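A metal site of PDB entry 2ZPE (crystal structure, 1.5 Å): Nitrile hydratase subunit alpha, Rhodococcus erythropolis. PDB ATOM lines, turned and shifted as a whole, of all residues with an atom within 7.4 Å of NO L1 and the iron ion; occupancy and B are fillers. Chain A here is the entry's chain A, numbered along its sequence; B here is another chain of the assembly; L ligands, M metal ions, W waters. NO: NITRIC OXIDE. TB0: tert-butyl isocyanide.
OG of Ser 113 sits at hydrogen-bond distance from O of NO L1.
OD2 of CSD 112 lies within salt-bridge range of NH1 of Arg 141 of chain B, at 2.8 Å.
The side-chain hydroxyl (OH) of Tyr 127 lies within hydrogen-bond range of the backbone NH (N) of Cys 109 (3.4 Å).
The side-chain hydroxyl (OG1) of Thr 115 sits at hydrogen-bond distance from the backbone carbonyl oxygen (O) of Ser 113.
OD1 of CSD 112 lies within salt-bridge range of NE of Arg 56 of chain B (2.9 Å).
The side-chain hydroxyl (OH) of Tyr 127 sits at hydrogen-bond distance from O of CSO 114.
The backbone carbonyl oxygen (O) of Thr 162 sits close to the side-chain sulfur (SG) of Cys 109, at 3.6 Å.
The side-chain hydroxyl of Tyr 72 of chain B lies within hydrogen-bond range of the side-chain hydroxyl of Ser 113 (2.6 Å).
SG of CSO 114 sits close to the guanidinium group of Arg 141 of chain B, at 3.7 Å.
The nearest printed residue that does not touch NO L1 is Gln 90 (4.3 Å).
Along chain A the residues within 4 Å of the iron ion span positions 109 to 114.
The nearest printed residue that does not touch the iron ion is Arg 141 of chain B (4.7 Å).
The iron ion is bound by N of CSO 114 (2.0 Å), a nitrogen (N) of NO L1 (2.0 Å), the backbone nitrogen (N) of Ser 113 (2.0 Å), SG of CSD 112 (2.2 Å), SG of CSO 114 (2.2 Å) and the side-chain sulfur (SG) of Cys 109 (2.4 Å).
Water W1 lies within hydrogen-bond range of OE1 of Gln 90 (2.8 Å), N of Thr 115 (3.0 Å), O of NO L1 (3.2 Å) and NE1 of Trp 117 (3.2 Å).
Water W2 lies within hydrogen-bond range of the side-chain hydroxyl of Ser 113, the indole nitrogen of Trp 117 and an oxygen (O) of NO L1.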
ATOM      1  N   GLN A  90      -0.200   1.271  10.094  1.00  0.00           N
ATOM      2  CA  GLN A  90       1.213   0.942  10.310  1.00  0.00           C
ATOM      3  C   GLN A  90       1.906   0.605   8.997  1.00  0.00           C
ATOM      4  O   GLN A  90       2.854  -0.182   8.938  1.00  0.00           O
ATOM      5  CB  GLN A  90       1.383  -0.181  11.347  1.00  0.00           C
ATOM      6  CG  GLN A  90       0.917   0.238  12.752  1.00  0.00           C
ATOM      7  CD  GLN A  90       1.642   1.463  13.233  1.00  0.00           C
ATOM      8  OE1 GLN A  90       2.869   1.451  13.329  1.00  0.00           O
ATOM      9  NE2 GLN A  90       0.913   2.528  13.516  1.00  0.00           N
ATOM     10  N   VAL A 108      14.433  -3.381  12.405  1.00  0.00           N
ATOM     11  CA  VAL A 108      14.034  -3.609  13.798  1.00  0.00           C
ATOM     12  C   VAL A 108      13.213  -2.408  14.266  1.00  0.00           C
ATOM     13  O   VAL A 108      13.232  -1.336  13.645  1.00  0.00           O
ATOM     14  CB  VAL A 108      15.291  -3.767  14.708  1.00  0.00           C
ATOM     15  CG1 VAL A 108      16.136  -2.469  14.725  1.00  0.00           C
ATOM     16  CG2 VAL A 108      14.907  -4.193  16.145  1.00  0.00           C
ATOM     17  N   CYS A 109      12.501  -2.587  15.385  1.00  0.00           N
ATOM     18  CA  CYS A 109      12.018  -1.453  16.181  1.00  0.00           C
ATOM     19  C   CYS A 109      12.598  -1.620  17.575  1.00  0.00           C
ATOM     20  O   CYS A 109      12.057  -2.380  18.406  1.00  0.00           O
ATOM     21  CB  CYS A 109      10.512  -1.431  16.253  1.00  0.00           C
ATOM     22  SG  CYS A 109       9.879  -0.060  17.252  1.00  0.00           S
ATOM     23  N   SER A 110      13.702  -0.934  17.860  1.00  0.00           N
ATOM     24  CA  SER A 110      14.363  -1.168  19.130  1.00  0.00           C
ATOM     25  C   SER A 110      13.499  -0.676  20.304  1.00  0.00           C
ATOM     26  O   SER A 110      13.614  -1.207  21.419  1.00  0.00           O
ATOM     27  CB  SER A 110      15.736  -0.508  19.183  1.00  0.00           C
ATOM     28  OG  SER A 110      15.641   0.904  19.242  1.00  0.00           O
ATOM     29  N   LEU A 111      12.646   0.323  20.055  1.00  0.00           N
ATOM     30  CA  LEU A 111      11.876   0.947  21.127  1.00  0.00           C
ATOM     31  C   LEU A 111      10.570   0.231  21.436  1.00  0.00           C
ATOM     32  O   LEU A 111       9.924   0.503  22.456  1.00  0.00           O
ATOM     33  CB  LEU A 111      11.593   2.411  20.770  1.00  0.00           C
ATOM     34  CG  LEU A 111      12.837   3.294  20.692  1.00  0.00           C
ATOM     35  CD1 LEU A 111      12.493   4.627  20.021  1.00  0.00           C
ATOM     36  CD2 LEU A 111      13.460   3.515  22.066  1.00  0.00           C
ATOM     37  N   CSD A 112      10.007  -0.758  20.468  1.00  0.00           N
ATOM     38  CA  CSD A 112       8.735  -1.396  20.715  1.00  0.00           C
ATOM     39  CB  CSD A 112       7.570  -0.381  20.698  1.00  0.00           C
ATOM     40  SG  CSD A 112       7.536   0.769  19.332  1.00  0.00           S
ATOM     41  C   CSD A 112       8.598  -2.473  19.673  1.00  0.00           C
ATOM     42  O   CSD A 112       8.980  -3.626  19.900  1.00  0.00           O
ATOM     43  OD1 CSD A 112       6.206   1.483  19.513  1.00  0.00           O
ATOM     44  OD2 CSD A 112       8.672   1.733  19.537  1.00  0.00           O
ATOM     45  N   SER A 113       7.908  -2.240  18.386  1.00  0.00           N
ATOM     46  CA  SER A 113       7.660  -3.440  17.536  1.00  0.00           C
ATOM     47  C   SER A 113       7.364  -2.990  16.125  1.00  0.00           C
ATOM     48  O   SER A 113       7.071  -3.798  15.237  1.00  0.00           O
ATOM     49  CB  SER A 113       6.472  -4.244  18.076  1.00  0.00           C
ATOM     50  OG  SER A 113       5.281  -3.461  18.008  1.00  0.00           O
ATOM     51  N   CSO A 114       7.549  -1.519  15.894  1.00  0.00           N
ATOM     52  CA  CSO A 114       7.132  -0.893  14.647  1.00  0.00           C
ATOM     53  CB  CSO A 114       7.675   0.520  14.617  1.00  0.00           C
ATOM     54  SG  CSO A 114       7.342   1.309  16.166  1.00  0.00           S
ATOM     55  C   CSO A 114       7.609  -1.726  13.463  1.00  0.00           C
ATOM     56  O   CSO A 114       8.740  -2.166  13.313  1.00  0.00           O
ATOM     57  OD  CSO A 114       5.862   1.707  16.002  1.00  0.00           O
ATOM     58  N   THR A 115       6.532  -2.049  12.554  1.00  0.00           N
ATOM     59  CA  THR A 115       6.558  -3.037  11.451  1.00  0.00           C
ATOM     60  C   THR A 115       5.556  -2.562  10.423  1.00  0.00           C
ATOM     61  O   THR A 115       4.507  -2.042  10.777  1.00  0.00           O
ATOM     62  CB  THR A 115       6.148  -4.423  11.981  1.00  0.00           C
ATOM     63  OG1 THR A 115       7.185  -4.922  12.847  1.00  0.00           O
ATOM     64  CG2 THR A 115       5.894  -5.427  10.854  1.00  0.00           C
ATOM     65  N   TRP A 117       2.941  -3.489   8.960  1.00  0.00           N
ATOM     66  CA  TRP A 117       1.892  -4.505   9.129  1.00  0.00           C
ATOM     67  C   TRP A 117       1.224  -5.012   7.851  1.00  0.00           C
ATOM     68  O   TRP A 117       1.084  -6.213   7.688  1.00  0.00           O
ATOM     69  CB  TRP A 117       0.770  -4.045  10.058  1.00  0.00           C
ATOM     70  CG  TRP A 117       1.118  -3.862  11.498  1.00  0.00           C
ATOM     71  CD1 TRP A 117       2.268  -4.237  12.148  1.00  0.00           C
ATOM     72  CD2 TRP A 117       0.248  -3.303  12.488  1.00  0.00           C
ATOM     73  NE1 TRP A 117       2.171  -3.907  13.494  1.00  0.00           N
ATOM     74  CE2 TRP A 117       0.939  -3.341  13.723  1.00  0.00           C
ATOM     75  CE3 TRP A 117      -1.048  -2.761  12.463  1.00  0.00           C
ATOM     76  CZ2 TRP A 117       0.382  -2.862  14.910  1.00  0.00           C
ATOM     77  CZ3 TRP A 117      -1.605  -2.283  13.649  1.00  0.00           C
ATOM     78  CH2 TRP A 117      -0.895  -2.341  14.853  1.00  0.00           C
ATOM     79  N   PRO A 123       4.176  -8.225  13.535  1.00  0.00           N
ATOM     80  CA  PRO A 123       5.497  -8.762  13.870  1.00  0.00           C
ATOM     81  C   PRO A 123       5.399 -10.068  14.656  1.00  0.00           C
ATOM     82  O   PRO A 123       4.485 -10.238  15.462  1.00  0.00           O
ATOM     83  CB  PRO A 123       6.128  -7.653  14.727  1.00  0.00           C
ATOM     84  CG  PRO A 123       4.977  -6.886  15.273  1.00  0.00           C
ATOM     85  CD  PRO A 123       3.965  -6.907  14.148  1.00  0.00           C
ATOM     86  N   TYR A 127      10.663 -10.928  16.951  1.00  0.00           N
ATOM     87  CA  TYR A 127      11.048  -9.593  16.491  1.00  0.00           C
ATOM     88  C   TYR A 127      10.804  -8.566  17.602  1.00  0.00           C
ATOM     89  O   TYR A 127      11.474  -7.525  17.684  1.00  0.00           O
ATOM     90  CB  TYR A 127      10.262  -9.257  15.226  1.00  0.00           C
ATOM     91  CG  TYR A 127      10.419  -7.869  14.640  1.00  0.00           C
ATOM     92  CD1 TYR A 127       9.628  -6.798  15.093  1.00  0.00           C
ATOM     93  CD2 TYR A 127      11.307  -7.638  13.588  1.00  0.00           C
ATOM     94  CE1 TYR A 127       9.732  -5.528  14.520  1.00  0.00           C
ATOM     95  CE2 TYR A 127      11.415  -6.385  13.015  1.00  0.00           C
ATOM     96  CZ  TYR A 127      10.638  -5.316  13.485  1.00  0.00           C
ATOM     97  OH  TYR A 127      10.719  -4.070  12.887  1.00  0.00           O
ATOM     98  N   LYS A 128       9.796  -8.864  18.420  1.00  0.00           N
ATOM     99  CA  LYS A 128       9.411  -8.021  19.552  1.00  0.00           C
ATOM    100  C   LYS A 128      10.201  -8.374  20.817  1.00  0.00           C
ATOM    101  O   LYS A 128      10.010  -7.738  21.856  1.00  0.00           O
ATOM    102  CB  LYS A 128       7.912  -8.172  19.822  1.00  0.00           C
ATOM    103  CG  LYS A 128       7.051  -7.704  18.661  1.00  0.00           C
ATOM    104  CD  LYS A 128       5.576  -8.016  18.852  1.00  0.00           C
ATOM    105  CE  LYS A 128       5.254  -9.466  18.587  1.00  0.00           C
ATOM    106  NZ  LYS A 128       3.785  -9.703  18.578  1.00  0.00           N
ATOM    107  N   ARG A 133      15.571  -6.653  19.986  1.00  0.00           N
ATOM    108  CA  ARG A 133      15.555  -5.210  20.160  1.00  0.00           C
ATOM    109  C   ARG A 133      16.863  -4.675  20.736  1.00  0.00           C
ATOM    110  O   ARG A 133      17.314  -3.603  20.349  1.00  0.00           O
ATOM    111  CB  ARG A 133      14.386  -4.832  21.078  1.00  0.00           C
ATOM    112  CG  ARG A 133      13.030  -5.019  20.383  1.00  0.00           C
ATOM    113  CD  ARG A 133      11.828  -4.750  21.286  1.00  0.00           C
ATOM    114  NE  ARG A 133      12.006  -3.491  21.996  1.00  0.00           N
ATOM    115  CZ  ARG A 133      11.374  -3.155  23.122  1.00  0.00           C
ATOM    116  NH1 ARG A 133      10.461  -3.956  23.657  1.00  0.00           N
ATOM    117  NH2 ARG A 133      11.659  -2.010  23.708  1.00  0.00           N
ATOM    118  N   THR A 162      13.188   1.413  13.272  1.00  0.00           N
ATOM    119  CA  THR A 162      11.909   1.988  12.891  1.00  0.00           C
ATOM    120  C   THR A 162      11.391   2.877  14.016  1.00  0.00           C
ATOM    121  O   THR A 162      10.564   2.454  14.818  1.00  0.00           O
ATOM    122  CB  THR A 162      10.902   0.879  12.539  1.00  0.00           C
ATOM    123  OG1 THR A 162      11.498  -0.007  11.575  1.00  0.00           O
ATOM    124  CG2 THR A 162       9.617   1.462  11.967  1.00  0.00           C
ATOM    125  N   THR A 163      11.897   4.099  14.066  1.00  0.00           N
ATOM    126  CA  THR A 163      11.696   4.995  15.204  1.00  0.00           C
ATOM    127  C   THR A 163      10.625   6.058  14.983  1.00  0.00           C
ATOM    128  O   THR A 163      10.264   6.772  15.925  1.00  0.00           O
ATOM    129  CB  THR A 163      13.021   5.690  15.569  1.00  0.00           C
ATOM    130  OG1 THR A 163      13.645   6.168  14.359  1.00  0.00           O
ATOM    131  CG2 THR A 163      13.972   4.720  16.248  1.00  0.00           C
ATOM    132  N   ARG A 167       7.749   3.031   7.413  1.00  0.00           N
ATOM    133  CA  ARG A 167       7.620   1.601   7.600  1.00  0.00           C
ATOM    134  C   ARG A 167       8.365   0.929   6.459  1.00  0.00           C
ATOM    135  O   ARG A 167       8.165   1.268   5.281  1.00  0.00           O
ATOM    136  CB  ARG A 167       6.145   1.198   7.658  1.00  0.00           C
ATOM    137  CG  ARG A 167       5.420   1.776   8.882  1.00  0.00           C
ATOM    138  CD  ARG A 167       5.791   1.033  10.178  1.00  0.00           C
ATOM    139  NE  ARG A 167       5.183   1.677  11.338  1.00  0.00           N
ATOM    140  CZ  ARG A 167       5.692   2.725  11.969  1.00  0.00           C
ATOM    141  NH1 ARG A 167       6.849   3.241  11.567  1.00  0.00           N
ATOM    142  NH2 ARG A 167       5.045   3.258  13.003  1.00  0.00           N
ATOM    143  N   TYR B  37      -4.649  -4.389  20.292  1.00  0.00           N
ATOM    144  CA  TYR B  37      -4.604  -3.563  19.082  1.00  0.00           C
ATOM    145  C   TYR B  37      -5.986  -3.076  18.672  1.00  0.00           C
ATOM    146  O   TYR B  37      -6.160  -1.901  18.304  1.00  0.00           O
ATOM    147  CB  TYR B  37      -3.967  -4.301  17.895  1.00  0.00           C
ATOM    148  CG  TYR B  37      -2.457  -4.505  17.927  1.00  0.00           C
ATOM    149  CD1 TYR B  37      -1.626  -3.900  18.891  1.00  0.00           C
ATOM    150  CD2 TYR B  37      -1.862  -5.291  16.941  1.00  0.00           C
ATOM    151  CE1 TYR B  37      -0.217  -4.103  18.857  1.00  0.00           C
ATOM    152  CE2 TYR B  37      -0.484  -5.484  16.906  1.00  0.00           C
ATOM    153  CZ  TYR B  37       0.316  -4.904  17.857  1.00  0.00           C
ATOM    154  OH  TYR B  37       1.677  -5.113  17.769  1.00  0.00           O
ATOM    155  N   VAL B  52      -1.876   7.250  18.911  1.00  0.00           N
ATOM    156  CA  VAL B  52      -0.998   6.087  18.934  1.00  0.00           C
ATOM    157  C   VAL B  52       0.253   6.412  19.772  1.00  0.00           C
ATOM    158  O   VAL B  52       0.747   5.570  20.529  1.00  0.00           O
ATOM    159  CB  VAL B  52      -0.612   5.608  17.508  1.00  0.00           C
ATOM    160  CG1 VAL B  52       0.366   4.450  17.581  1.00  0.00           C
ATOM    161  CG2 VAL B  52      -1.852   5.168  16.728  1.00  0.00           C
ATOM    162  N   ARG B  56       2.261   4.362  22.872  1.00  0.00           N
ATOM    163  CA  ARG B  56       3.685   4.053  23.063  1.00  0.00           C
ATOM    164  C   ARG B  56       4.154   4.570  24.423  1.00  0.00           C
ATOM    165  O   ARG B  56       4.832   3.841  25.169  1.00  0.00           O
ATOM    166  CB  ARG B  56       4.535   4.678  21.961  1.00  0.00           C
ATOM    167  CG  ARG B  56       4.272   4.147  20.572  1.00  0.00           C
ATOM    168  CD  ARG B  56       5.385   4.502  19.607  1.00  0.00           C
ATOM    169  NE  ARG B  56       5.101   3.897  18.304  1.00  0.00           N
ATOM    170  CZ  ARG B  56       4.356   4.484  17.363  1.00  0.00           C
ATOM    171  NH1 ARG B  56       3.859   5.712  17.570  1.00  0.00           N
ATOM    172  NH2 ARG B  56       4.115   3.843  16.229  1.00  0.00           N
ATOM    173  N   TYR B  72       4.751  -9.096  25.431  1.00  0.00           N
ATOM    174  CA  TYR B  72       4.372  -8.017  24.539  1.00  0.00           C
ATOM    175  C   TYR B  72       2.883  -7.648  24.554  1.00  0.00           C
ATOM    176  O   TYR B  72       2.536  -6.514  24.878  1.00  0.00           O
ATOM    177  CB  TYR B  72       4.827  -8.321  23.100  1.00  0.00           C
ATOM    178  CG  TYR B  72       4.440  -7.233  22.138  1.00  0.00           C
ATOM    179  CD1 TYR B  72       5.277  -6.142  21.904  1.00  0.00           C
ATOM    180  CD2 TYR B  72       3.213  -7.284  21.468  1.00  0.00           C
ATOM    181  CE1 TYR B  72       4.913  -5.131  21.037  1.00  0.00           C
ATOM    182  CE2 TYR B  72       2.838  -6.287  20.584  1.00  0.00           C
ATOM    183  CZ  TYR B  72       3.682  -5.200  20.379  1.00  0.00           C
ATOM    184  OH  TYR B  72       3.362  -4.190  19.521  1.00  0.00           O
ATOM    185  N   TYR B  76       0.317  -4.042  26.136  1.00  0.00           N
ATOM    186  CA  TYR B  76      -0.669  -3.174  25.474  1.00  0.00           C
ATOM    187  C   TYR B  76      -2.056  -3.259  26.088  1.00  0.00           C
ATOM    188  O   TYR B  76      -2.774  -2.266  26.090  1.00  0.00           O
ATOM    189  CB  TYR B  76      -0.656  -3.378  23.937  1.00  0.00           C
ATOM    190  CG  TYR B  76       0.682  -2.919  23.395  1.00  0.00           C
ATOM    191  CD1 TYR B  76       0.898  -1.610  22.950  1.00  0.00           C
ATOM    192  CD2 TYR B  76       1.778  -3.765  23.466  1.00  0.00           C
ATOM    193  CE1 TYR B  76       2.176  -1.180  22.518  1.00  0.00           C
ATOM    194  CE2 TYR B  76       3.045  -3.349  23.067  1.00  0.00           C
ATOM    195  CZ  TYR B  76       3.230  -2.060  22.592  1.00  0.00           C
ATOM    196  OH  TYR B  76       4.505  -1.683  22.210  1.00  0.00           O
ATOM    197  N   ARG B 141      11.034   9.970  20.474  1.00  0.00           N
ATOM    198  CA  ARG B 141      11.341   8.917  19.503  1.00  0.00           C
ATOM    199  C   ARG B 141      12.793   8.960  19.054  1.00  0.00           C
ATOM    200  O   ARG B 141      13.136   8.788  17.885  1.00  0.00           O
ATOM    201  CB  ARG B 141      10.370   8.975  18.305  1.00  0.00           C
ATOM    202  CG  ARG B 141       8.940   8.611  18.689  1.00  0.00           C
ATOM    203  CD  ARG B 141       8.902   7.264  19.415  1.00  0.00           C
ATOM    204  NE  ARG B 141       9.137   6.178  18.481  1.00  0.00           N
ATOM    205  CZ  ARG B 141       9.083   4.892  18.802  1.00  0.00           C
ATOM    206  NH1 ARG B 141       8.876   4.522  20.069  1.00  0.00           N
ATOM    207  NH2 ARG B 141       9.265   3.972  17.864  1.00  0.00           N
HETATM  208  N    NO L   1       5.627  -0.586  17.786  1.00  0.00           N
HETATM  209  O    NO L   1       4.671  -0.440  16.713  1.00  0.00           O
HETATM  210  C   TB0 L   2      -0.786  -0.061  19.816  1.00  0.00           C
HETATM  211  N   TB0 L   2       0.183   0.077  19.203  1.00  0.00           N
HETATM  212  C2  TB0 L   2       1.378   0.187  18.415  1.00  0.00           C
HETATM  213  C4  TB0 L   2       2.050  -1.182  18.449  1.00  0.00           C
HETATM  214  C3  TB0 L   2       2.289   1.260  19.011  1.00  0.00           C
HETATM  215  C1  TB0 L   2       0.988   0.574  16.983  1.00  0.00           C
HETATM  216 FE    FE M   1       7.571  -0.447  17.526  1.00  0.00          FE
HETATM  217  O   HOH W   1       3.893  -1.176  13.735  1.00  0.00           O
HETATM  218  O   HOH W   2       4.283  -3.306  15.399  1.00  0.00           O
